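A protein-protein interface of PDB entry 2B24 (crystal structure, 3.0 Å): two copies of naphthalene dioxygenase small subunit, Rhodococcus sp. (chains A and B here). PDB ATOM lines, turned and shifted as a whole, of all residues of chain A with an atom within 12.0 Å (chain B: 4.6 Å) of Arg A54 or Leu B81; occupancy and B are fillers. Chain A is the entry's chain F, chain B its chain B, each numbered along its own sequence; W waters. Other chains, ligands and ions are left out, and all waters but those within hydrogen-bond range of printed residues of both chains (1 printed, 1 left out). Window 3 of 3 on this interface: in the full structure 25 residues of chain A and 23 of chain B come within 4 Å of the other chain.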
ATOM      1  N   ARG A  49      -1.013  -8.216   7.063  1.00  0.00           N
ATOM      2  CA  ARG A  49      -0.605  -7.172   6.157  1.00  0.00           C
ATOM      3  C   ARG A  49       0.415  -7.796   5.230  1.00  0.00           C
ATOM      4  O   ARG A  49       1.164  -8.670   5.648  1.00  0.00           O
ATOM      5  CB  ARG A  49       0.094  -6.091   6.954  1.00  0.00           C
ATOM      6  CG  ARG A  49      -0.770  -4.997   7.480  1.00  0.00           C
ATOM      7  CD  ARG A  49      -0.442  -3.706   6.818  1.00  0.00           C
ATOM      8  NE  ARG A  49       0.125  -2.713   7.703  1.00  0.00           N
ATOM      9  CZ  ARG A  49       0.046  -1.421   7.455  1.00  0.00           C
ATOM     10  NH1 ARG A  49      -0.583  -1.002   6.379  1.00  0.00           N
ATOM     11  NH2 ARG A  49       0.566  -0.542   8.281  1.00  0.00           N
ATOM     12  N   VAL A  50       0.454  -7.356   3.977  1.00  0.00           N
ATOM     13  CA  VAL A  50       1.474  -7.797   3.028  1.00  0.00           C
ATOM     14  C   VAL A  50       1.992  -6.567   2.313  1.00  0.00           C
ATOM     15  O   VAL A  50       1.265  -5.603   2.179  1.00  0.00           O
ATOM     16  CB  VAL A  50       0.959  -8.843   1.987  1.00  0.00           C
ATOM     17  CG1 VAL A  50       0.591 -10.169   2.642  1.00  0.00           C
ATOM     18  CG2 VAL A  50      -0.203  -8.303   1.175  1.00  0.00           C
ATOM     19  N   THR A  51       3.255  -6.593   1.886  1.00  0.00           N
ATOM     20  CA  THR A  51       3.833  -5.533   1.064  1.00  0.00           C
ATOM     21  C   THR A  51       3.179  -5.546  -0.300  1.00  0.00           C
ATOM     22  O   THR A  51       3.190  -6.553  -0.991  1.00  0.00           O
ATOM     23  CB  THR A  51       5.316  -5.734   0.878  1.00  0.00           C
ATOM     24  OG1 THR A  51       5.861  -6.274   2.069  1.00  0.00           O
ATOM     25  CG2 THR A  51       6.011  -4.415   0.747  1.00  0.00           C
ATOM     26  N   ARG A  52       2.586  -4.420  -0.658  1.00  0.00           N
ATOM     27  CA  ARG A  52       2.019  -4.216  -1.963  1.00  0.00           C
ATOM     28  C   ARG A  52       2.461  -2.825  -2.374  1.00  0.00           C
ATOM     29  O   ARG A  52       3.012  -2.087  -1.568  1.00  0.00           O
ATOM     30  CB  ARG A  52       0.493  -4.308  -1.909  1.00  0.00           C
ATOM     31  CG  ARG A  52      -0.018  -5.647  -1.454  1.00  0.00           C
ATOM     32  CD  ARG A  52      -1.192  -6.183  -2.240  1.00  0.00           C
ATOM     33  NE  ARG A  52      -0.870  -6.269  -3.651  1.00  0.00           N
ATOM     34  CZ  ARG A  52      -1.717  -6.643  -4.596  1.00  0.00           C
ATOM     35  NH1 ARG A  52      -2.957  -6.993  -4.287  1.00  0.00           N
ATOM     36  NH2 ARG A  52      -1.318  -6.667  -5.861  1.00  0.00           N
ATOM     37  N   GLU A  53       2.222  -2.464  -3.626  1.00  0.00           N
ATOM     38  CA  GLU A  53       2.595  -1.155  -4.124  1.00  0.00           C
ATOM     39  C   GLU A  53       1.570  -0.095  -3.707  1.00  0.00           C
ATOM     40  O   GLU A  53       0.431  -0.430  -3.370  1.00  0.00           O
ATOM     41  CB  GLU A  53       2.741  -1.217  -5.640  1.00  0.00           C
ATOM     42  CG  GLU A  53       2.333  -2.548  -6.217  1.00  0.00           C
ATOM     43  CD  GLU A  53       1.087  -2.440  -7.061  1.00  0.00           C
ATOM     44  OE1 GLU A  53       0.552  -3.512  -7.441  1.00  0.00           O
ATOM     45  OE2 GLU A  53       0.654  -1.292  -7.367  1.00  0.00           O
ATOM     46  N   ARG A  54       1.978   1.175  -3.727  1.00  0.00           N
ATOM     47  CA  ARG A  54       1.073   2.295  -3.477  1.00  0.00           C
ATOM     48  C   ARG A  54      -0.205   2.229  -4.333  1.00  0.00           C
ATOM     49  O   ARG A  54      -1.314   2.378  -3.817  1.00  0.00           O
ATOM     50  CB  ARG A  54       1.799   3.613  -3.723  1.00  0.00           C
ATOM     51  CG  ARG A  54       1.929   4.522  -2.494  1.00  0.00           C
ATOM     52  CD  ARG A  54       2.380   5.946  -2.852  1.00  0.00           C
ATOM     53  NE  ARG A  54       3.306   6.616  -1.921  1.00  0.00           N
ATOM     54  CZ  ARG A  54       3.115   6.772  -0.612  1.00  0.00           C
ATOM     55  NH1 ARG A  54       2.051   6.239  -0.017  1.00  0.00           N
ATOM     56  NH2 ARG A  54       4.008   7.446   0.110  1.00  0.00           N
ATOM     57  N   GLU A  55      -0.039   1.994  -5.634  1.00  0.00           N
ATOM     58  CA  GLU A  55      -1.151   1.842  -6.578  1.00  0.00           C
ATOM     59  C   GLU A  55      -2.276   0.966  -6.029  1.00  0.00           C
ATOM     60  O   GLU A  55      -3.417   1.432  -5.920  1.00  0.00           O
ATOM     61  CB  GLU A  55      -0.647   1.265  -7.913  1.00  0.00           C
ATOM     62  CG  GLU A  55      -1.625   1.373  -9.082  1.00  0.00           C
ATOM     63  CD  GLU A  55      -1.161   0.601 -10.319  1.00  0.00           C
ATOM     64  OE1 GLU A  55      -1.788   0.764 -11.405  1.00  0.00           O
ATOM     65  OE2 GLU A  55      -0.170  -0.178 -10.203  1.00  0.00           O
ATOM     66  N   ALA A  56      -1.933  -0.282  -5.676  1.00  0.00           N
ATOM     67  CA  ALA A  56      -2.888  -1.337  -5.266  1.00  0.00           C
ATOM     68  C   ALA A  56      -3.891  -0.840  -4.252  1.00  0.00           C
ATOM     69  O   ALA A  56      -3.557  -0.004  -3.420  1.00  0.00           O
ATOM     70  CB  ALA A  56      -2.145  -2.558  -4.711  1.00  0.00           C
ATOM     71  N   VAL A  57      -5.107  -1.368  -4.325  1.00  0.00           N
ATOM     72  CA  VAL A  57      -6.222  -0.912  -3.487  1.00  0.00           C
ATOM     73  C   VAL A  57      -5.922  -0.851  -1.988  1.00  0.00           C
ATOM     74  O   VAL A  57      -6.258   0.129  -1.336  1.00  0.00           O
ATOM     75  CB  VAL A  57      -7.508  -1.760  -3.690  1.00  0.00           C
ATOM     76  CG1 VAL A  57      -8.699  -0.852  -3.927  1.00  0.00           C
ATOM     77  CG2 VAL A  57      -7.347  -2.775  -4.828  1.00  0.00           C
ATOM     78  N   THR A  58      -5.289  -1.893  -1.452  1.00  0.00           N
ATOM     79  CA  THR A  58      -5.094  -2.037  -0.014  1.00  0.00           C
ATOM     80  C   THR A  58      -3.938  -2.960   0.380  1.00  0.00           C
ATOM     81  O   THR A  58      -3.478  -3.793  -0.390  1.00  0.00           O
ATOM     82  CB  THR A  58      -6.406  -2.513   0.650  1.00  0.00           C
ATOM     83  OG1 THR A  58      -6.231  -2.596   2.063  1.00  0.00           O
ATOM     84  CG2 THR A  58      -6.728  -3.944   0.267  1.00  0.00           C
ATOM     85  N   ASP A  59      -3.509  -2.806   1.623  1.00  0.00           N
ATOM     86  CA  ASP A  59      -2.413  -3.556   2.224  1.00  0.00           C
ATOM     87  C   ASP A  59      -2.921  -4.789   2.931  1.00  0.00           C
ATOM     88  O   ASP A  59      -2.268  -5.813   2.950  1.00  0.00           O
ATOM     89  CB  ASP A  59      -1.762  -2.676   3.279  1.00  0.00           C
ATOM     90  CG  ASP A  59      -0.294  -2.596   3.123  1.00  0.00           C
ATOM     91  OD1 ASP A  59       0.354  -2.101   4.056  1.00  0.00           O
ATOM     92  OD2 ASP A  59       0.308  -2.990   2.111  1.00  0.00           O
ATOM     93  N   VAL A  60      -4.098  -4.653   3.526  1.00  0.00           N
ATOM     94  CA  VAL A  60      -4.632  -5.600   4.482  1.00  0.00           C
ATOM     95  C   VAL A  60      -5.258  -6.790   3.782  1.00  0.00           C
ATOM     96  O   VAL A  60      -6.115  -6.635   2.919  1.00  0.00           O
ATOM     97  CB  VAL A  60      -5.681  -4.915   5.390  1.00  0.00           C
ATOM     98  CG1 VAL A  60      -6.143  -5.843   6.472  1.00  0.00           C
ATOM     99  CG2 VAL A  60      -5.126  -3.668   6.012  1.00  0.00           C
ATOM    100  N   GLY B  29       0.283   7.844   4.555  1.00  0.00           N
ATOM    101  CA  GLY B  29       0.883   8.093   3.262  1.00  0.00           C
ATOM    102  C   GLY B  29       0.351   9.315   2.546  1.00  0.00           C
ATOM    103  O   GLY B  29       0.758   9.606   1.436  1.00  0.00           O
ATOM    104  N   TYR B  31       0.767  12.450   2.039  1.00  0.00           N
ATOM    105  CA  TYR B  31       1.723  13.545   2.090  1.00  0.00           C
ATOM    106  C   TYR B  31       1.184  14.813   1.436  1.00  0.00           C
ATOM    107  O   TYR B  31       1.429  15.906   1.924  1.00  0.00           O
ATOM    108  CB  TYR B  31       3.051  13.116   1.461  1.00  0.00           C
ATOM    109  CG  TYR B  31       3.878  12.252   2.373  1.00  0.00           C
ATOM    110  CD1 TYR B  31       3.778  10.881   2.344  1.00  0.00           C
ATOM    111  CD2 TYR B  31       4.753  12.809   3.272  1.00  0.00           C
ATOM    112  CE1 TYR B  31       4.545  10.086   3.202  1.00  0.00           C
ATOM    113  CE2 TYR B  31       5.510  12.025   4.122  1.00  0.00           C
ATOM    114  CZ  TYR B  31       5.402  10.673   4.089  1.00  0.00           C
ATOM    115  OH  TYR B  31       6.154   9.916   4.949  1.00  0.00           O
ATOM    116  N   ARG B  77       9.264  17.346  -2.844  1.00  0.00           N
ATOM    117  CA  ARG B  77       9.440  16.097  -2.126  1.00  0.00           C
ATOM    118  C   ARG B  77       8.173  15.289  -2.158  1.00  0.00           C
ATOM    119  O   ARG B  77       8.228  14.081  -2.168  1.00  0.00           O
ATOM    120  CB  ARG B  77       9.852  16.366  -0.679  1.00  0.00           C
ATOM    121  CG  ARG B  77       9.924  15.115   0.183  1.00  0.00           C
ATOM    122  CD  ARG B  77      10.923  15.177   1.309  1.00  0.00           C
ATOM    123  NE  ARG B  77      11.905  16.235   1.089  1.00  0.00           N
ATOM    124  CZ  ARG B  77      13.206  16.033   0.979  1.00  0.00           C
ATOM    125  NH1 ARG B  77      13.697  14.806   1.070  1.00  0.00           N
ATOM    126  NH2 ARG B  77      14.014  17.064   0.778  1.00  0.00           N
ATOM    127  N   VAL B  78       7.034  15.965  -2.159  1.00  0.00           N
ATOM    128  CA  VAL B  78       5.744  15.300  -2.174  1.00  0.00           C
ATOM    129  C   VAL B  78       5.402  14.976  -3.621  1.00  0.00           C
ATOM    130  O   VAL B  78       4.926  13.883  -3.915  1.00  0.00           O
ATOM    131  CB  VAL B  78       4.656  16.159  -1.505  1.00  0.00           C
ATOM    132  CG1 VAL B  78       3.293  15.542  -1.708  1.00  0.00           C
ATOM    133  CG2 VAL B  78       4.944  16.327  -0.015  1.00  0.00           C
ATOM    134  N   LEU B  79       5.686  15.920  -4.521  1.00  0.00           N
ATOM    135  CA  LEU B  79       5.547  15.738  -5.971  1.00  0.00           C
ATOM    136  C   LEU B  79       6.255  14.489  -6.474  1.00  0.00           C
ATOM    137  O   LEU B  79       5.752  13.813  -7.348  1.00  0.00           O
ATOM    138  CB  LEU B  79       6.101  16.956  -6.707  1.00  0.00           C
ATOM    139  CG  LEU B  79       5.237  17.782  -7.657  1.00  0.00           C
ATOM    140  CD1 LEU B  79       3.823  17.260  -7.797  1.00  0.00           C
ATOM    141  CD2 LEU B  79       5.219  19.220  -7.229  1.00  0.00           C
ATOM    142  N   ARG B  80       7.424  14.196  -5.913  1.00  0.00           N
ATOM    143  CA  ARG B  80       8.216  13.039  -6.283  1.00  0.00           C
ATOM    144  C   ARG B  80       7.514  11.766  -5.895  1.00  0.00           C
ATOM    145  O   ARG B  80       7.582  10.788  -6.610  1.00  0.00           O
ATOM    146  CB  ARG B  80       9.558  13.096  -5.589  1.00  0.00           C
ATOM    147  CG  ARG B  80      10.611  12.283  -6.241  1.00  0.00           C
ATOM    148  CD  ARG B  80      11.820  12.077  -5.375  1.00  0.00           C
ATOM    149  NE  ARG B  80      11.673  10.964  -4.446  1.00  0.00           N
ATOM    150  CZ  ARG B  80      11.982   9.717  -4.731  1.00  0.00           C
ATOM    151  NH1 ARG B  80      12.450   9.424  -5.923  1.00  0.00           N
ATOM    152  NH2 ARG B  80      11.830   8.772  -3.826  1.00  0.00           N
ATOM    153  N   LEU B  81       6.838  11.783  -4.756  1.00  0.00           N
ATOM    154  CA  LEU B  81       6.179  10.599  -4.221  1.00  0.00           C
ATOM    155  C   LEU B  81       4.822  10.328  -4.886  1.00  0.00           C
ATOM    156  O   LEU B  81       4.275   9.237  -4.772  1.00  0.00           O
ATOM    157  CB  LEU B  81       6.023  10.734  -2.698  1.00  0.00           C
ATOM    158  CG  LEU B  81       7.276  10.848  -1.817  1.00  0.00           C
ATOM    159  CD1 LEU B  81       6.945  11.598  -0.551  1.00  0.00           C
ATOM    160  CD2 LEU B  81       7.855   9.502  -1.472  1.00  0.00           C
ATOM    161  N   GLU B  82       4.297  11.334  -5.579  1.00  0.00           N
ATOM    162  CA  GLU B  82       3.029  11.244  -6.299  1.00  0.00           C
ATOM    163  C   GLU B  82       3.222  10.682  -7.680  1.00  0.00           C
ATOM    164  O   GLU B  82       2.275  10.266  -8.332  1.00  0.00           O
ATOM    165  CB  GLU B  82       2.385  12.612  -6.408  1.00  0.00           C
ATOM    166  CG  GLU B  82       1.837  13.118  -5.094  1.00  0.00           C
ATOM    167  CD  GLU B  82       1.348  14.524  -5.192  1.00  0.00           C
ATOM    168  OE1 GLU B  82       0.445  14.879  -4.444  1.00  0.00           O
ATOM    169  OE2 GLU B  82       1.857  15.273  -6.022  1.00  0.00           O
ATOM    170  N   THR B  83       4.467  10.703  -8.126  1.00  0.00           N
ATOM    171  CA  THR B  83       4.884  10.028  -9.335  1.00  0.00           C
ATOM    172  C   THR B  83       4.888   8.527  -9.050  1.00  0.00           C
ATOM    173  O   THR B  83       4.935   8.117  -7.893  1.00  0.00           O
ATOM    174  CB  THR B  83       6.254  10.561  -9.773  1.00  0.00           C
ATOM    175  OG1 THR B  83       6.330  10.511 -11.192  1.00  0.00           O
ATOM    176  CG2 THR B  83       7.367   9.656  -9.360  1.00  0.00           C
ATOM    177  N   ALA B  86       8.827   6.316  -7.564  1.00  0.00           N
ATOM    178  CA  ALA B  86       9.495   6.724  -6.346  1.00  0.00           C
ATOM    179  C   ALA B  86       9.889   5.495  -5.565  1.00  0.00           C
ATOM    180  O   ALA B  86       9.339   5.237  -4.509  1.00  0.00           O
ATOM    181  CB  ALA B  86       8.583   7.613  -5.516  1.00  0.00           C
ATOM    182  N   GLU B  89       9.976   4.523  -1.819  1.00  0.00           N
ATOM    183  CA  GLU B  89       8.725   4.400  -1.091  1.00  0.00           C
ATOM    184  C   GLU B  89       7.553   3.857  -1.919  1.00  0.00           C
ATOM    185  O   GLU B  89       6.400   4.051  -1.503  1.00  0.00           O
ATOM    186  CB  GLU B  89       8.328   5.757  -0.497  1.00  0.00           C
ATOM    187  CG  GLU B  89       9.140   6.211   0.710  1.00  0.00           C
ATOM    188  CD  GLU B  89       8.825   5.434   1.969  1.00  0.00           C
ATOM    189  OE1 GLU B  89       7.641   5.270   2.312  1.00  0.00           O
ATOM    190  OE2 GLU B  89       9.767   4.986   2.630  1.00  0.00           O
ATOM    191  N   ASP B  90       7.823   3.185  -3.055  1.00  0.00           N
ATOM    192  CA  ASP B  90       6.722   2.811  -3.966  1.00  0.00           C
ATOM    193  C   ASP B  90       6.030   1.482  -3.778  1.00  0.00           C
ATOM    194  O   ASP B  90       4.864   1.341  -4.208  1.00  0.00           O
ATOM    195  CB  ASP B  90       6.966   3.052  -5.443  1.00  0.00           C
ATOM    196  CG  ASP B  90       5.664   3.338  -6.186  1.00  0.00           C
ATOM    197  OD1 ASP B  90       4.642   2.659  -5.911  1.00  0.00           O
ATOM    198  OD2 ASP B  90       5.564   4.241  -7.045  1.00  0.00           O
ATOM    199  N   PRO B  92       5.392   1.119  -0.317  1.00  0.00           N
ATOM    200  CA  PRO B  92       5.572   2.079   0.774  1.00  0.00           C
ATOM    201  C   PRO B  92       5.990   1.456   2.079  1.00  0.00           C
ATOM    202  O   PRO B  92       5.641   0.311   2.352  1.00  0.00           O
ATOM    203  CB  PRO B  92       4.180   2.646   0.964  1.00  0.00           C
ATOM    204  CG  PRO B  92       3.433   2.220  -0.155  1.00  0.00           C
ATOM    205  CD  PRO B  92       3.968   0.941  -0.626  1.00  0.00           C
HETATM  206  O   HOH W   1       4.697   5.851   2.669  1.00  0.00           O
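The backbone carbonyl oxygen (O) of Asp B90 lies within hydrogen-bond range of the backbone NH (N) of Arg A54 (2.9 Å).
The guanidinium group (NH2) of Arg A52 lies within salt-bridge range of the side-chain carboxylate (OE1) of Glu A53 (3.99 Å). N of Ala A56 lies within hydrogen-bond range of OE2 of Glu A53.
Arg A52 touches Pro B92 (O to CD, 3.3 Å). Glu A53 touches Asp B90 (CA to O, 3.4 Å). O of Gly B29 touches NH1 of Arg A54 (3.9 Å). Arg A54 touches Leu B81 (NE to O, 3.99 Å). Arg A54 touches Pro B92.
Printed residues of chain B within 4 Å of Arg A54: Gly B29 (3.9 Å), Leu B81 (3.99 Å), Asp B90 (2.9 Å) and Pro B92 (3.6 Å). Printed residues of chain A within 4 Å of Leu B81: Arg A54 (3.99 Å). No residue of chain A comes within 4 Å of Tyr B31. No residue of chain A comes within 4 Å of Val B78. No residue of chain A comes within 4 Å of Arg B80. No residue of chain A comes within 4 Å of Glu B82. No residue of chain A comes within 4 Å of Glu B89. Asp B90 touches two residues of chain A. Of the printed residues of chain B, Glu A53 touches Asp B90. Printed residues of chain B within 4 Å of Arg A52: Pro B92. Ala A56 touches none of the printed residues of chain B. The nearest printed residue of chain A that does not touch Leu B81 is Glu A55 (8.5 Å). The nearest printed residue of chain B that does not touch Glu A53 is Pro B92 (4.04 Å).
Of the 13 printed residues of chain B, 4 touch a printed residue of chain A. Printed residues of chain B that touch a printed residue of chain A: Gly B29, Leu B81, Asp B90 and Pro B92. Among the printed residues, no Asp or Glu carboxylate lies within 4 Å of a Lys or Arg side-chain nitrogen of the other chain.
No position is printed for both chains. Of the 6 pairs that touch across the chains among the printed residues, none has its exchanged pair printed and touching as well.
Water W1 bridges OE1 of Glu B89 and NH2 of Arg A54.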
